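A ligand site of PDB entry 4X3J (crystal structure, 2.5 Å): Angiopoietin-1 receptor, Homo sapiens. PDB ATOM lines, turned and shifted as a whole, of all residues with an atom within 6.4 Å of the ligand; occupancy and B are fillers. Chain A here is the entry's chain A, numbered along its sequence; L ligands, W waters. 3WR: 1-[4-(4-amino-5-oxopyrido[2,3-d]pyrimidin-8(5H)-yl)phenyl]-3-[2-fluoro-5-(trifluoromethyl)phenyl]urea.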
ATOM      1  N   VAL A  37      35.778 -20.722 -32.729  1.00  0.00           N
ATOM      2  CA  VAL A  37      34.556 -20.718 -31.913  1.00  0.00           C
ATOM      3  C   VAL A  37      34.367 -19.350 -31.246  1.00  0.00           C
ATOM      4  O   VAL A  37      35.082 -19.009 -30.308  1.00  0.00           O
ATOM      5  CB  VAL A  37      34.461 -21.912 -30.913  1.00  0.00           C
ATOM      6  CG1 VAL A  37      33.200 -21.808 -30.040  1.00  0.00           C
ATOM      7  CG2 VAL A  37      34.485 -23.241 -31.637  1.00  0.00           C
ATOM      8  N   ALA A  51      24.172 -17.149 -29.185  1.00  0.00           N
ATOM      9  CA  ALA A  51      24.753 -18.299 -29.879  1.00  0.00           C
ATOM     10  C   ALA A  51      26.268 -18.328 -29.773  1.00  0.00           C
ATOM     11  O   ALA A  51      26.894 -17.337 -29.370  1.00  0.00           O
ATOM     12  CB  ALA A  51      24.324 -18.303 -31.338  1.00  0.00           C
ATOM     13  N   ALA A  52      26.847 -19.491 -30.078  1.00  0.00           N
ATOM     14  CA  ALA A  52      28.283 -19.759 -30.124  1.00  0.00           C
ATOM     15  C   ALA A  52      28.489 -20.451 -31.466  1.00  0.00           C
ATOM     16  O   ALA A  52      27.990 -21.571 -31.672  1.00  0.00           O
ATOM     17  CB  ALA A  52      28.696 -20.657 -28.971  1.00  0.00           C
ATOM     18  N   LYS A  54      30.666 -22.134 -34.509  1.00  0.00           N
ATOM     19  CA  LYS A  54      31.870 -22.945 -34.712  1.00  0.00           C
ATOM     20  C   LYS A  54      32.655 -22.489 -35.946  1.00  0.00           C
ATOM     21  O   LYS A  54      32.085 -22.232 -37.013  1.00  0.00           O
ATOM     22  CB  LYS A  54      31.520 -24.439 -34.795  1.00  0.00           C
ATOM     23  CG  LYS A  54      32.645 -25.318 -34.273  1.00  0.00           C
ATOM     24  CD  LYS A  54      32.312 -26.811 -34.271  1.00  0.00           C
ATOM     25  CE  LYS A  54      33.477 -27.631 -33.774  1.00  0.00           C
ATOM     26  NZ  LYS A  54      33.801 -27.331 -32.342  1.00  0.00           N
ATOM     27  N   GLU A  71      29.430 -33.505 -36.246  1.00  0.00           N
ATOM     28  CA  GLU A  71      28.666 -33.252 -35.030  1.00  0.00           C
ATOM     29  C   GLU A  71      27.297 -32.605 -35.289  1.00  0.00           C
ATOM     30  O   GLU A  71      26.459 -32.577 -34.390  1.00  0.00           O
ATOM     31  CB  GLU A  71      29.481 -32.441 -33.985  1.00  0.00           C
ATOM     32  CG  GLU A  71      29.874 -31.011 -34.325  1.00  0.00           C
ATOM     33  CD  GLU A  71      31.117 -30.570 -33.593  1.00  0.00           C
ATOM     34  OE1 GLU A  71      32.227 -30.792 -34.128  1.00  0.00           O
ATOM     35  OE2 GLU A  71      30.996 -30.066 -32.447  1.00  0.00           O
ATOM     36  N   LEU A  72      27.097 -32.084 -36.520  1.00  0.00           N
ATOM     37  CA  LEU A  72      25.878 -31.414 -36.994  1.00  0.00           C
ATOM     38  C   LEU A  72      24.601 -32.270 -36.799  1.00  0.00           C
ATOM     39  O   LEU A  72      23.600 -31.761 -36.279  1.00  0.00           O
ATOM     40  CB  LEU A  72      26.071 -30.999 -38.473  1.00  0.00           C
ATOM     41  CG  LEU A  72      24.860 -30.434 -39.239  1.00  0.00           C
ATOM     42  CD1 LEU A  72      24.406 -29.098 -38.686  1.00  0.00           C
ATOM     43  CD2 LEU A  72      25.184 -30.298 -40.711  1.00  0.00           C
ATOM     44  N   VAL A  74      24.294 -35.072 -34.812  1.00  0.00           N
ATOM     45  CA  VAL A  74      24.288 -35.368 -33.370  1.00  0.00           C
ATOM     46  C   VAL A  74      23.470 -34.327 -32.555  1.00  0.00           C
ATOM     47  O   VAL A  74      22.607 -34.714 -31.758  1.00  0.00           O
ATOM     48  CB  VAL A  74      25.764 -35.519 -32.874  1.00  0.00           C
ATOM     49  CG1 VAL A  74      25.878 -35.426 -31.357  1.00  0.00           C
ATOM     50  CG2 VAL A  74      26.407 -36.798 -33.396  1.00  0.00           C
ATOM     51  N   LEU A  75      23.718 -33.033 -32.784  1.00  0.00           N
ATOM     52  CA  LEU A  75      23.059 -31.944 -32.071  1.00  0.00           C
ATOM     53  C   LEU A  75      21.566 -31.736 -32.427  1.00  0.00           C
ATOM     54  O   LEU A  75      20.785 -31.339 -31.558  1.00  0.00           O
ATOM     55  CB  LEU A  75      23.849 -30.646 -32.228  1.00  0.00           C
ATOM     56  CG  LEU A  75      25.343 -30.740 -31.856  1.00  0.00           C
ATOM     57  CD1 LEU A  75      26.116 -29.547 -32.386  1.00  0.00           C
ATOM     58  CD2 LEU A  75      25.544 -30.922 -30.358  1.00  0.00           C
ATOM     59  N   LEU A  78      19.808 -35.628 -31.388  1.00  0.00           N
ATOM     60  CA  LEU A  78      19.730 -35.786 -29.927  1.00  0.00           C
ATOM     61  C   LEU A  78      18.979 -34.578 -29.357  1.00  0.00           C
ATOM     62  O   LEU A  78      19.477 -33.859 -28.472  1.00  0.00           O
ATOM     63  CB  LEU A  78      21.122 -35.992 -29.285  1.00  0.00           C
ATOM     64  CG  LEU A  78      21.970 -37.187 -29.766  1.00  0.00           C
ATOM     65  CD1 LEU A  78      23.413 -37.030 -29.338  1.00  0.00           C
ATOM     66  CD2 LEU A  78      21.420 -38.513 -29.268  1.00  0.00           C
ATOM     67  N   ILE A  84      21.493 -31.570 -22.801  1.00  0.00           N
ATOM     68  CA  ILE A  84      22.371 -31.847 -23.930  1.00  0.00           C
ATOM     69  C   ILE A  84      22.464 -30.551 -24.719  1.00  0.00           C
ATOM     70  O   ILE A  84      21.436 -29.961 -25.039  1.00  0.00           O
ATOM     71  CB  ILE A  84      21.874 -33.050 -24.790  1.00  0.00           C
ATOM     72  CG1 ILE A  84      22.229 -34.367 -24.103  1.00  0.00           C
ATOM     73  CG2 ILE A  84      22.470 -33.050 -26.207  1.00  0.00           C
ATOM     74  CD1 ILE A  84      21.068 -35.126 -23.680  1.00  0.00           C
ATOM     75  N   ILE A  85      23.691 -30.092 -25.004  1.00  0.00           N
ATOM     76  CA  ILE A  85      23.864 -28.870 -25.791  1.00  0.00           C
ATOM     77  C   ILE A  85      23.122 -28.997 -27.148  1.00  0.00           C
ATOM     78  O   ILE A  85      23.205 -30.031 -27.803  1.00  0.00           O
ATOM     79  CB  ILE A  85      25.352 -28.442 -25.907  1.00  0.00           C
ATOM     80  CG1 ILE A  85      25.487 -26.925 -26.060  1.00  0.00           C
ATOM     81  CG2 ILE A  85      26.116 -29.195 -26.998  1.00  0.00           C
ATOM     82  CD1 ILE A  85      25.310 -26.086 -24.722  1.00  0.00           C
ATOM     83  N   ILE A 101      25.568 -23.187 -32.070  1.00  0.00           N
ATOM     84  CA  ILE A 101      25.334 -24.030 -30.895  1.00  0.00           C
ATOM     85  C   ILE A 101      24.703 -23.123 -29.847  1.00  0.00           C
ATOM     86  O   ILE A 101      25.004 -21.931 -29.831  1.00  0.00           O
ATOM     87  CB  ILE A 101      26.659 -24.667 -30.344  1.00  0.00           C
ATOM     88  CG1 ILE A 101      27.476 -25.371 -31.458  1.00  0.00           C
ATOM     89  CG2 ILE A 101      26.386 -25.650 -29.215  1.00  0.00           C
ATOM     90  CD1 ILE A 101      28.981 -25.149 -31.351  1.00  0.00           C
ATOM     91  N   GLU A 102      23.826 -23.676 -28.984  1.00  0.00           N
ATOM     92  CA  GLU A 102      23.221 -22.885 -27.918  1.00  0.00           C
ATOM     93  C   GLU A 102      24.323 -22.417 -26.968  1.00  0.00           C
ATOM     94  O   GLU A 102      25.186 -23.213 -26.559  1.00  0.00           O
ATOM     95  CB  GLU A 102      22.039 -23.574 -27.221  1.00  0.00           C
ATOM     96  CG  GLU A 102      22.341 -24.838 -26.448  1.00  0.00           C
ATOM     97  CD  GLU A 102      21.304 -25.208 -25.402  1.00  0.00           C
ATOM     98  OE1 GLU A 102      20.874 -26.383 -25.391  1.00  0.00           O
ATOM     99  OE2 GLU A 102      20.927 -24.326 -24.593  1.00  0.00           O
ATOM    100  N   TYR A 103      24.377 -21.097 -26.753  1.00  0.00           N
ATOM    101  CA  TYR A 103      25.406 -20.491 -25.931  1.00  0.00           C
ATOM    102  C   TYR A 103      25.220 -20.764 -24.453  1.00  0.00           C
ATOM    103  O   TYR A 103      24.120 -20.615 -23.923  1.00  0.00           O
ATOM    104  CB  TYR A 103      25.514 -18.969 -26.219  1.00  0.00           C
ATOM    105  CG  TYR A 103      26.499 -18.235 -25.337  1.00  0.00           C
ATOM    106  CD1 TYR A 103      27.872 -18.414 -25.478  1.00  0.00           C
ATOM    107  CD2 TYR A 103      26.055 -17.352 -24.359  1.00  0.00           C
ATOM    108  CE1 TYR A 103      28.776 -17.758 -24.653  1.00  0.00           C
ATOM    109  CE2 TYR A 103      26.961 -16.661 -23.542  1.00  0.00           C
ATOM    110  CZ  TYR A 103      28.317 -16.874 -23.684  1.00  0.00           C
ATOM    111  OH  TYR A 103      29.196 -16.208 -22.870  1.00  0.00           O
ATOM    112  N   ALA A 104      26.322 -21.164 -23.807  1.00  0.00           N
ATOM    113  CA  ALA A 104      26.422 -21.394 -22.372  1.00  0.00           C
ATOM    114  C   ALA A 104      27.148 -20.157 -21.771  1.00  0.00           C
ATOM    115  O   ALA A 104      28.314 -19.914 -22.101  1.00  0.00           O
ATOM    116  CB  ALA A 104      27.192 -22.669 -22.098  1.00  0.00           C
ATOM    117  N   PRO A 105      26.487 -19.333 -20.936  1.00  0.00           N
ATOM    118  CA  PRO A 105      27.154 -18.127 -20.409  1.00  0.00           C
ATOM    119  C   PRO A 105      28.131 -18.314 -19.247  1.00  0.00           C
ATOM    120  O   PRO A 105      28.837 -17.355 -18.903  1.00  0.00           O
ATOM    121  CB  PRO A 105      25.977 -17.240 -20.000  1.00  0.00           C
ATOM    122  CG  PRO A 105      24.906 -18.204 -19.612  1.00  0.00           C
ATOM    123  CD  PRO A 105      25.084 -19.429 -20.466  1.00  0.00           C
ATOM    124  N   HIS A 106      28.156 -19.502 -18.619  1.00  0.00           N
ATOM    125  CA  HIS A 106      29.028 -19.762 -17.472  1.00  0.00           C
ATOM    126  C   HIS A 106      30.204 -20.674 -17.803  1.00  0.00           C
ATOM    127  O   HIS A 106      30.926 -21.120 -16.908  1.00  0.00           O
ATOM    128  CB  HIS A 106      28.203 -20.286 -16.282  1.00  0.00           C
ATOM    129  CG  HIS A 106      26.952 -19.484 -16.058  1.00  0.00           C
ATOM    130  ND1 HIS A 106      27.000 -18.238 -15.445  1.00  0.00           N
ATOM    131  CD2 HIS A 106      25.678 -19.743 -16.424  1.00  0.00           C
ATOM    132  CE1 HIS A 106      25.752 -17.794 -15.450  1.00  0.00           C
ATOM    133  NE2 HIS A 106      24.921 -18.669 -16.023  1.00  0.00           N
ATOM    134  N   GLY A 107      30.385 -20.891 -19.098  1.00  0.00           N
ATOM    135  CA  GLY A 107      31.444 -21.743 -19.655  1.00  0.00           C
ATOM    136  C   GLY A 107      31.346 -23.181 -19.223  1.00  0.00           C
ATOM    137  O   GLY A 107      30.269 -23.637 -18.804  1.00  0.00           O
ATOM    138  N   ASN A 108      32.462 -23.920 -19.324  1.00  0.00           N
ATOM    139  CA  ASN A 108      32.523 -25.329 -18.940  1.00  0.00           C
ATOM    140  C   ASN A 108      32.471 -25.516 -17.413  1.00  0.00           C
ATOM    141  O   ASN A 108      32.877 -24.613 -16.664  1.00  0.00           O
ATOM    142  CB  ASN A 108      33.703 -26.049 -19.590  1.00  0.00           C
ATOM    143  CG  ASN A 108      35.042 -25.813 -18.927  1.00  0.00           C
ATOM    144  OD1 ASN A 108      35.360 -26.420 -17.898  1.00  0.00           O
ATOM    145  ND2 ASN A 108      35.854 -24.970 -19.510  1.00  0.00           N
ATOM    146  N   LEU A 154      20.786 -40.181 -23.507  1.00  0.00           N
ATOM    147  CA  LEU A 154      21.802 -40.658 -24.444  1.00  0.00           C
ATOM    148  C   LEU A 154      21.785 -42.164 -24.569  1.00  0.00           C
ATOM    149  O   LEU A 154      21.658 -42.652 -25.681  1.00  0.00           O
ATOM    150  CB  LEU A 154      23.193 -40.093 -24.104  1.00  0.00           C
ATOM    151  CG  LEU A 154      23.411 -38.609 -24.481  1.00  0.00           C
ATOM    152  CD1 LEU A 154      24.885 -38.254 -24.507  1.00  0.00           C
ATOM    153  CD2 LEU A 154      22.789 -38.258 -25.834  1.00  0.00           C
ATOM    154  N   PHE A 159      23.247 -44.019 -27.748  1.00  0.00           N
ATOM    155  CA  PHE A 159      24.386 -43.158 -28.028  1.00  0.00           C
ATOM    156  C   PHE A 159      25.445 -43.278 -26.925  1.00  0.00           C
ATOM    157  O   PHE A 159      25.147 -43.052 -25.748  1.00  0.00           O
ATOM    158  CB  PHE A 159      23.895 -41.705 -28.202  1.00  0.00           C
ATOM    159  CG  PHE A 159      24.960 -40.767 -28.719  1.00  0.00           C
ATOM    160  CD1 PHE A 159      25.842 -40.135 -27.839  1.00  0.00           C
ATOM    161  CD2 PHE A 159      25.105 -40.534 -30.078  1.00  0.00           C
ATOM    162  CE1 PHE A 159      26.862 -39.318 -28.321  1.00  0.00           C
ATOM    163  CE2 PHE A 159      26.129 -39.711 -30.555  1.00  0.00           C
ATOM    164  CZ  PHE A 159      26.988 -39.097 -29.672  1.00  0.00           C
ATOM    165  N   HIS A 161      28.880 -41.672 -25.487  1.00  0.00           N
ATOM    166  CA  HIS A 161      29.576 -40.399 -25.477  1.00  0.00           C
ATOM    167  C   HIS A 161      31.079 -40.521 -25.762  1.00  0.00           C
ATOM    168  O   HIS A 161      31.582 -39.758 -26.586  1.00  0.00           O
ATOM    169  CB  HIS A 161      29.314 -39.644 -24.156  1.00  0.00           C
ATOM    170  CG  HIS A 161      29.762 -38.216 -24.203  1.00  0.00           C
ATOM    171  ND1 HIS A 161      31.120 -37.881 -24.185  1.00  0.00           N
ATOM    172  CD2 HIS A 161      29.032 -37.080 -24.296  1.00  0.00           C
ATOM    173  CE1 HIS A 161      31.165 -36.557 -24.260  1.00  0.00           C
ATOM    174  NE2 HIS A 161      29.942 -36.032 -24.308  1.00  0.00           N
ATOM    175  N   ASN A 168      33.758 -31.146 -20.368  1.00  0.00           N
ATOM    176  CA  ASN A 168      32.820 -31.368 -21.468  1.00  0.00           C
ATOM    177  C   ASN A 168      31.363 -31.056 -21.116  1.00  0.00           C
ATOM    178  O   ASN A 168      30.464 -31.292 -21.931  1.00  0.00           O
ATOM    179  CB  ASN A 168      32.939 -32.794 -22.026  1.00  0.00           C
ATOM    180  CG  ASN A 168      33.929 -32.941 -23.142  1.00  0.00           C
ATOM    181  OD1 ASN A 168      34.749 -33.862 -23.134  1.00  0.00           O
ATOM    182  ND2 ASN A 168      33.892 -32.051 -24.124  1.00  0.00           N
ATOM    183  N   LEU A 170      28.803 -28.020 -20.004  1.00  0.00           N
ATOM    184  CA  LEU A 170      28.678 -26.575 -20.049  1.00  0.00           C
ATOM    185  C   LEU A 170      27.644 -26.142 -19.019  1.00  0.00           C
ATOM    186  O   LEU A 170      26.664 -26.845 -18.801  1.00  0.00           O
ATOM    187  CB  LEU A 170      28.317 -26.115 -21.472  1.00  0.00           C
ATOM    188  CG  LEU A 170      29.469 -26.243 -22.529  1.00  0.00           C
ATOM    189  CD1 LEU A 170      28.956 -26.149 -23.933  1.00  0.00           C
ATOM    190  CD2 LEU A 170      30.564 -25.185 -22.306  1.00  0.00           C
ATOM    191  N   ILE A 179      25.507 -31.423 -21.431  1.00  0.00           N
ATOM    192  CA  ILE A 179      26.463 -32.376 -21.990  1.00  0.00           C
ATOM    193  C   ILE A 179      26.879 -31.883 -23.368  1.00  0.00           C
ATOM    194  O   ILE A 179      26.033 -31.505 -24.176  1.00  0.00           O
ATOM    195  CB  ILE A 179      25.899 -33.830 -22.023  1.00  0.00           C
ATOM    196  CG1 ILE A 179      25.758 -34.402 -20.576  1.00  0.00           C
ATOM    197  CG2 ILE A 179      26.740 -34.763 -22.940  1.00  0.00           C
ATOM    198  CD1 ILE A 179      24.749 -35.447 -20.442  1.00  0.00           C
ATOM    199  N   ALA A 180      28.204 -31.854 -23.601  1.00  0.00           N
ATOM    200  CA  ALA A 180      28.810 -31.428 -24.856  1.00  0.00           C
ATOM    201  C   ALA A 180      30.032 -32.331 -25.162  1.00  0.00           C
ATOM    202  O   ALA A 180      30.315 -33.257 -24.384  1.00  0.00           O
ATOM    203  CB  ALA A 180      29.238 -29.962 -24.738  1.00  0.00           C
ATOM    204  N   ASP A 181      30.706 -32.093 -26.309  1.00  0.00           N
ATOM    205  CA  ASP A 181      31.895 -32.826 -26.738  1.00  0.00           C
ATOM    206  C   ASP A 181      32.703 -31.970 -27.722  1.00  0.00           C
ATOM    207  O   ASP A 181      32.399 -31.907 -28.926  1.00  0.00           O
ATOM    208  CB  ASP A 181      31.579 -34.230 -27.285  1.00  0.00           C
ATOM    209  CG  ASP A 181      32.807 -35.133 -27.431  1.00  0.00           C
ATOM    210  OD1 ASP A 181      33.921 -34.704 -27.029  1.00  0.00           O
ATOM    211  OD2 ASP A 181      32.659 -36.263 -27.935  1.00  0.00           O
ATOM    212  N   PHE A 182      33.727 -31.304 -27.176  1.00  0.00           N
ATOM    213  CA  PHE A 182      34.630 -30.368 -27.853  1.00  0.00           C
ATOM    214  C   PHE A 182      36.052 -30.445 -27.279  1.00  0.00           C
ATOM    215  O   PHE A 182      36.245 -30.854 -26.121  1.00  0.00           O
ATOM    216  CB  PHE A 182      34.074 -28.930 -27.726  1.00  0.00           C
ATOM    217  CG  PHE A 182      33.852 -28.419 -26.317  1.00  0.00           C
ATOM    218  CD1 PHE A 182      32.621 -28.571 -25.693  1.00  0.00           C
ATOM    219  CD2 PHE A 182      34.872 -27.760 -25.630  1.00  0.00           C
ATOM    220  CE1 PHE A 182      32.425 -28.116 -24.381  1.00  0.00           C
ATOM    221  CE2 PHE A 182      34.665 -27.297 -24.321  1.00  0.00           C
ATOM    222  CZ  PHE A 182      33.445 -27.487 -23.710  1.00  0.00           C
ATOM    223  N   GLY A 183      37.017 -29.999 -28.090  1.00  0.00           N
ATOM    224  CA  GLY A 183      38.432 -29.942 -27.743  1.00  0.00           C
ATOM    225  C   GLY A 183      39.144 -28.724 -28.315  1.00  0.00           C
ATOM    226  O   GLY A 183      38.711 -27.582 -28.122  1.00  0.00           O
HETATM  227  C1  3WR L   1      30.537 -23.739 -26.165  1.00  0.00           C
HETATM  228  C3  3WR L   1      30.972 -22.945 -25.050  1.00  0.00           C
HETATM  229  C7  3WR L   1      32.328 -23.166 -24.531  1.00  0.00           C
HETATM  230  C8  3WR L   1      30.064 -21.991 -24.505  1.00  0.00           C
HETATM  231  C9  3WR L   1      28.471 -22.634 -26.097  1.00  0.00           C
HETATM  232  C10 3WR L   1      31.760 -26.274 -28.545  1.00  0.00           C
HETATM  233  C11 3WR L   1      29.723 -26.448 -27.278  1.00  0.00           C
HETATM  234  C12 3WR L   1      33.157 -24.110 -25.203  1.00  0.00           C
HETATM  235  C16 3WR L   1      31.365 -27.371 -29.310  1.00  0.00           C
HETATM  236  C20 3WR L   1      29.498 -30.326 -29.329  1.00  0.00           C
HETATM  237  C24 3WR L   1      28.150 -33.062 -28.804  1.00  0.00           C
HETATM  238  C27 3WR L   1      29.525 -35.073 -30.176  1.00  0.00           C
HETATM  239  C30 3WR L   1      27.042 -34.702 -27.320  1.00  0.00           C
HETATM  240  N2  3WR L   1      31.378 -24.734 -26.673  1.00  0.00           N
HETATM  241  N4  3WR L   1      29.279 -23.527 -26.635  1.00  0.00           N
HETATM  242  C5  3WR L   1      30.927 -25.779 -27.528  1.00  0.00           C
HETATM  243  C6  3WR L   1      32.676 -24.810 -26.251  1.00  0.00           C
HETATM  244  O13 3WR L   1      32.773 -22.551 -23.562  1.00  0.00           O
HETATM  245  N14 3WR L   1      28.850 -21.873 -25.073  1.00  0.00           N
HETATM  246  N15 3WR L   1      30.403 -21.174 -23.439  1.00  0.00           N
HETATM  247  C17 3WR L   1      29.305 -27.529 -28.048  1.00  0.00           C
HETATM  248  C18 3WR L   1      30.124 -27.987 -29.082  1.00  0.00           C
HETATM  249  N19 3WR L   1      29.793 -29.114 -29.868  1.00  0.00           N
HETATM  250  N21 3WR L   1      29.290 -31.370 -30.185  1.00  0.00           N
HETATM  251  O22 3WR L   1      29.406 -30.465 -28.125  1.00  0.00           O
HETATM  252  C23 3WR L   1      29.047 -32.709 -29.811  1.00  0.00           C
HETATM  253  C25 3WR L   1      29.727 -33.735 -30.494  1.00  0.00           C
HETATM  254  C26 3WR L   1      27.957 -34.393 -28.468  1.00  0.00           C
HETATM  255  F28 3WR L   1      30.601 -33.414 -31.467  1.00  0.00           F
HETATM  256  C29 3WR L   1      28.658 -35.400 -29.137  1.00  0.00           C
HETATM  257  F31 3WR L   1      25.901 -33.888 -27.370  1.00  0.00           F
HETATM  258  F32 3WR L   1      26.700 -36.059 -27.305  1.00  0.00           F
HETATM  259  F33 3WR L   1      27.760 -34.452 -26.152  1.00  0.00           F
HETATM  260  O   HOH W   1      30.515 -37.903 -28.296  1.00  0.00           O
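NZ of Lys 54 lies within salt-bridge range of OE2 of Glu 71 (3.9 Å).
The backbone carbonyl oxygen (O) of Ala 180 sits at hydrogen-bond distance from a ring nitrogen (NE2) of His 161 (2.8 Å).
The backbone NH (N) of Ala 180 is in hydrogen-bond range of the backbone carbonyl oxygen (O) of Asn 168, at 2.9 Å.
The backbone carbonyl oxygen (O) of Ile 179 is in hydrogen-bond range of the backbone NH (N) of Ile 85, at 2.9 Å.
The backbone carbonyl oxygen of Leu 154 is in hydrogen-bond range of the backbone NH of Phe 159.
O of Ala 52 lies within hydrogen-bond range of N of Ile 101, at 2.9 Å.
The side-chain amide nitrogen (ND2) of Asn 168 sits close to the backbone NH (N) of Phe 182.
Water W1 lies within hydrogen-bond range of the side-chain carboxylate (OD2) of Asp 181 (2.7 Å) and the backbone carbonyl oxygen (O) of His 161 (2.7 Å).
O22 of the ligand is in hydrogen-bond range of N of Asp 181, 2.8 Å away.
The backbone carbonyl oxygen of Asp 181 sits close to a nitrogen (N21) of the ligand (3.4 Å).
A nitrogen (N14) of the ligand lies within hydrogen-bond range of the backbone NH (N) of Ala 104, at 2.9 Å.
O of Ala 104 sits at hydrogen-bond distance from N15 of the ligand (2.8 Å).
OE2 of Glu 71 sits at hydrogen-bond distance from N19 of the ligand, at 3.0 Å.
NE2 of His 161 sits close to F33 of the ligand, at 3.3 Å.
The backbone carbonyl oxygen (O) of Ala 180 lies close to a fluorine (F33) of the ligand, at 3.3 Å.
Ala 52 touches the ligand.
Lys 54 touches the ligand (NZ to C16, 3.9 Å).
Val 74 touches the ligand (CG1 to C29, 3.6 Å).
CD2 of Leu 75 touches C24 of the ligand, at 3.7 Å.
Leu 78 touches the ligand (CD1 to F32, 3.99 Å).
CG2 of Ile 84 touches F31 of the ligand, at 3.7 Å.
CG2 of Ile 85 touches O22 of the ligand, at 3.7 Å.
Ile 101 touches the ligand.
O of Glu 102 touches C9 of the ligand, 3.4 Å away.
CD1 of Tyr 103 touches N14 of the ligand, 3.6 Å away.
CA of Gly 107 touches N15 of the ligand (3.97 Å).
CD1 of Leu 154 touches F32 of the ligand (3.99 Å).
CE1 of Phe 159 touches F32 of the ligand, at 3.4 Å.
Leu 170 touches the ligand (CD1 to C11, 3.4 Å).
CG2 of Ile 179 touches F33 of the ligand, at 3.4 Å.
Phe 182 touches the ligand (CB to C16, 3.5 Å).
Hydrophobic or aromatic side chains that line the ligand: Ala 52, Val 74, Leu 75, Leu 78, Ile 84, Ile 85, Ile 101, Tyr 103, Ala 104, Leu 154, Phe 159, His 161, Leu 170, Ile 179, Ala 180 and Phe 182.
Of the 29 residues printed, 21 come within 4 Å of the ligand.
Along chain A the residues within 4 Å of the ligand span positions 52 to 182.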
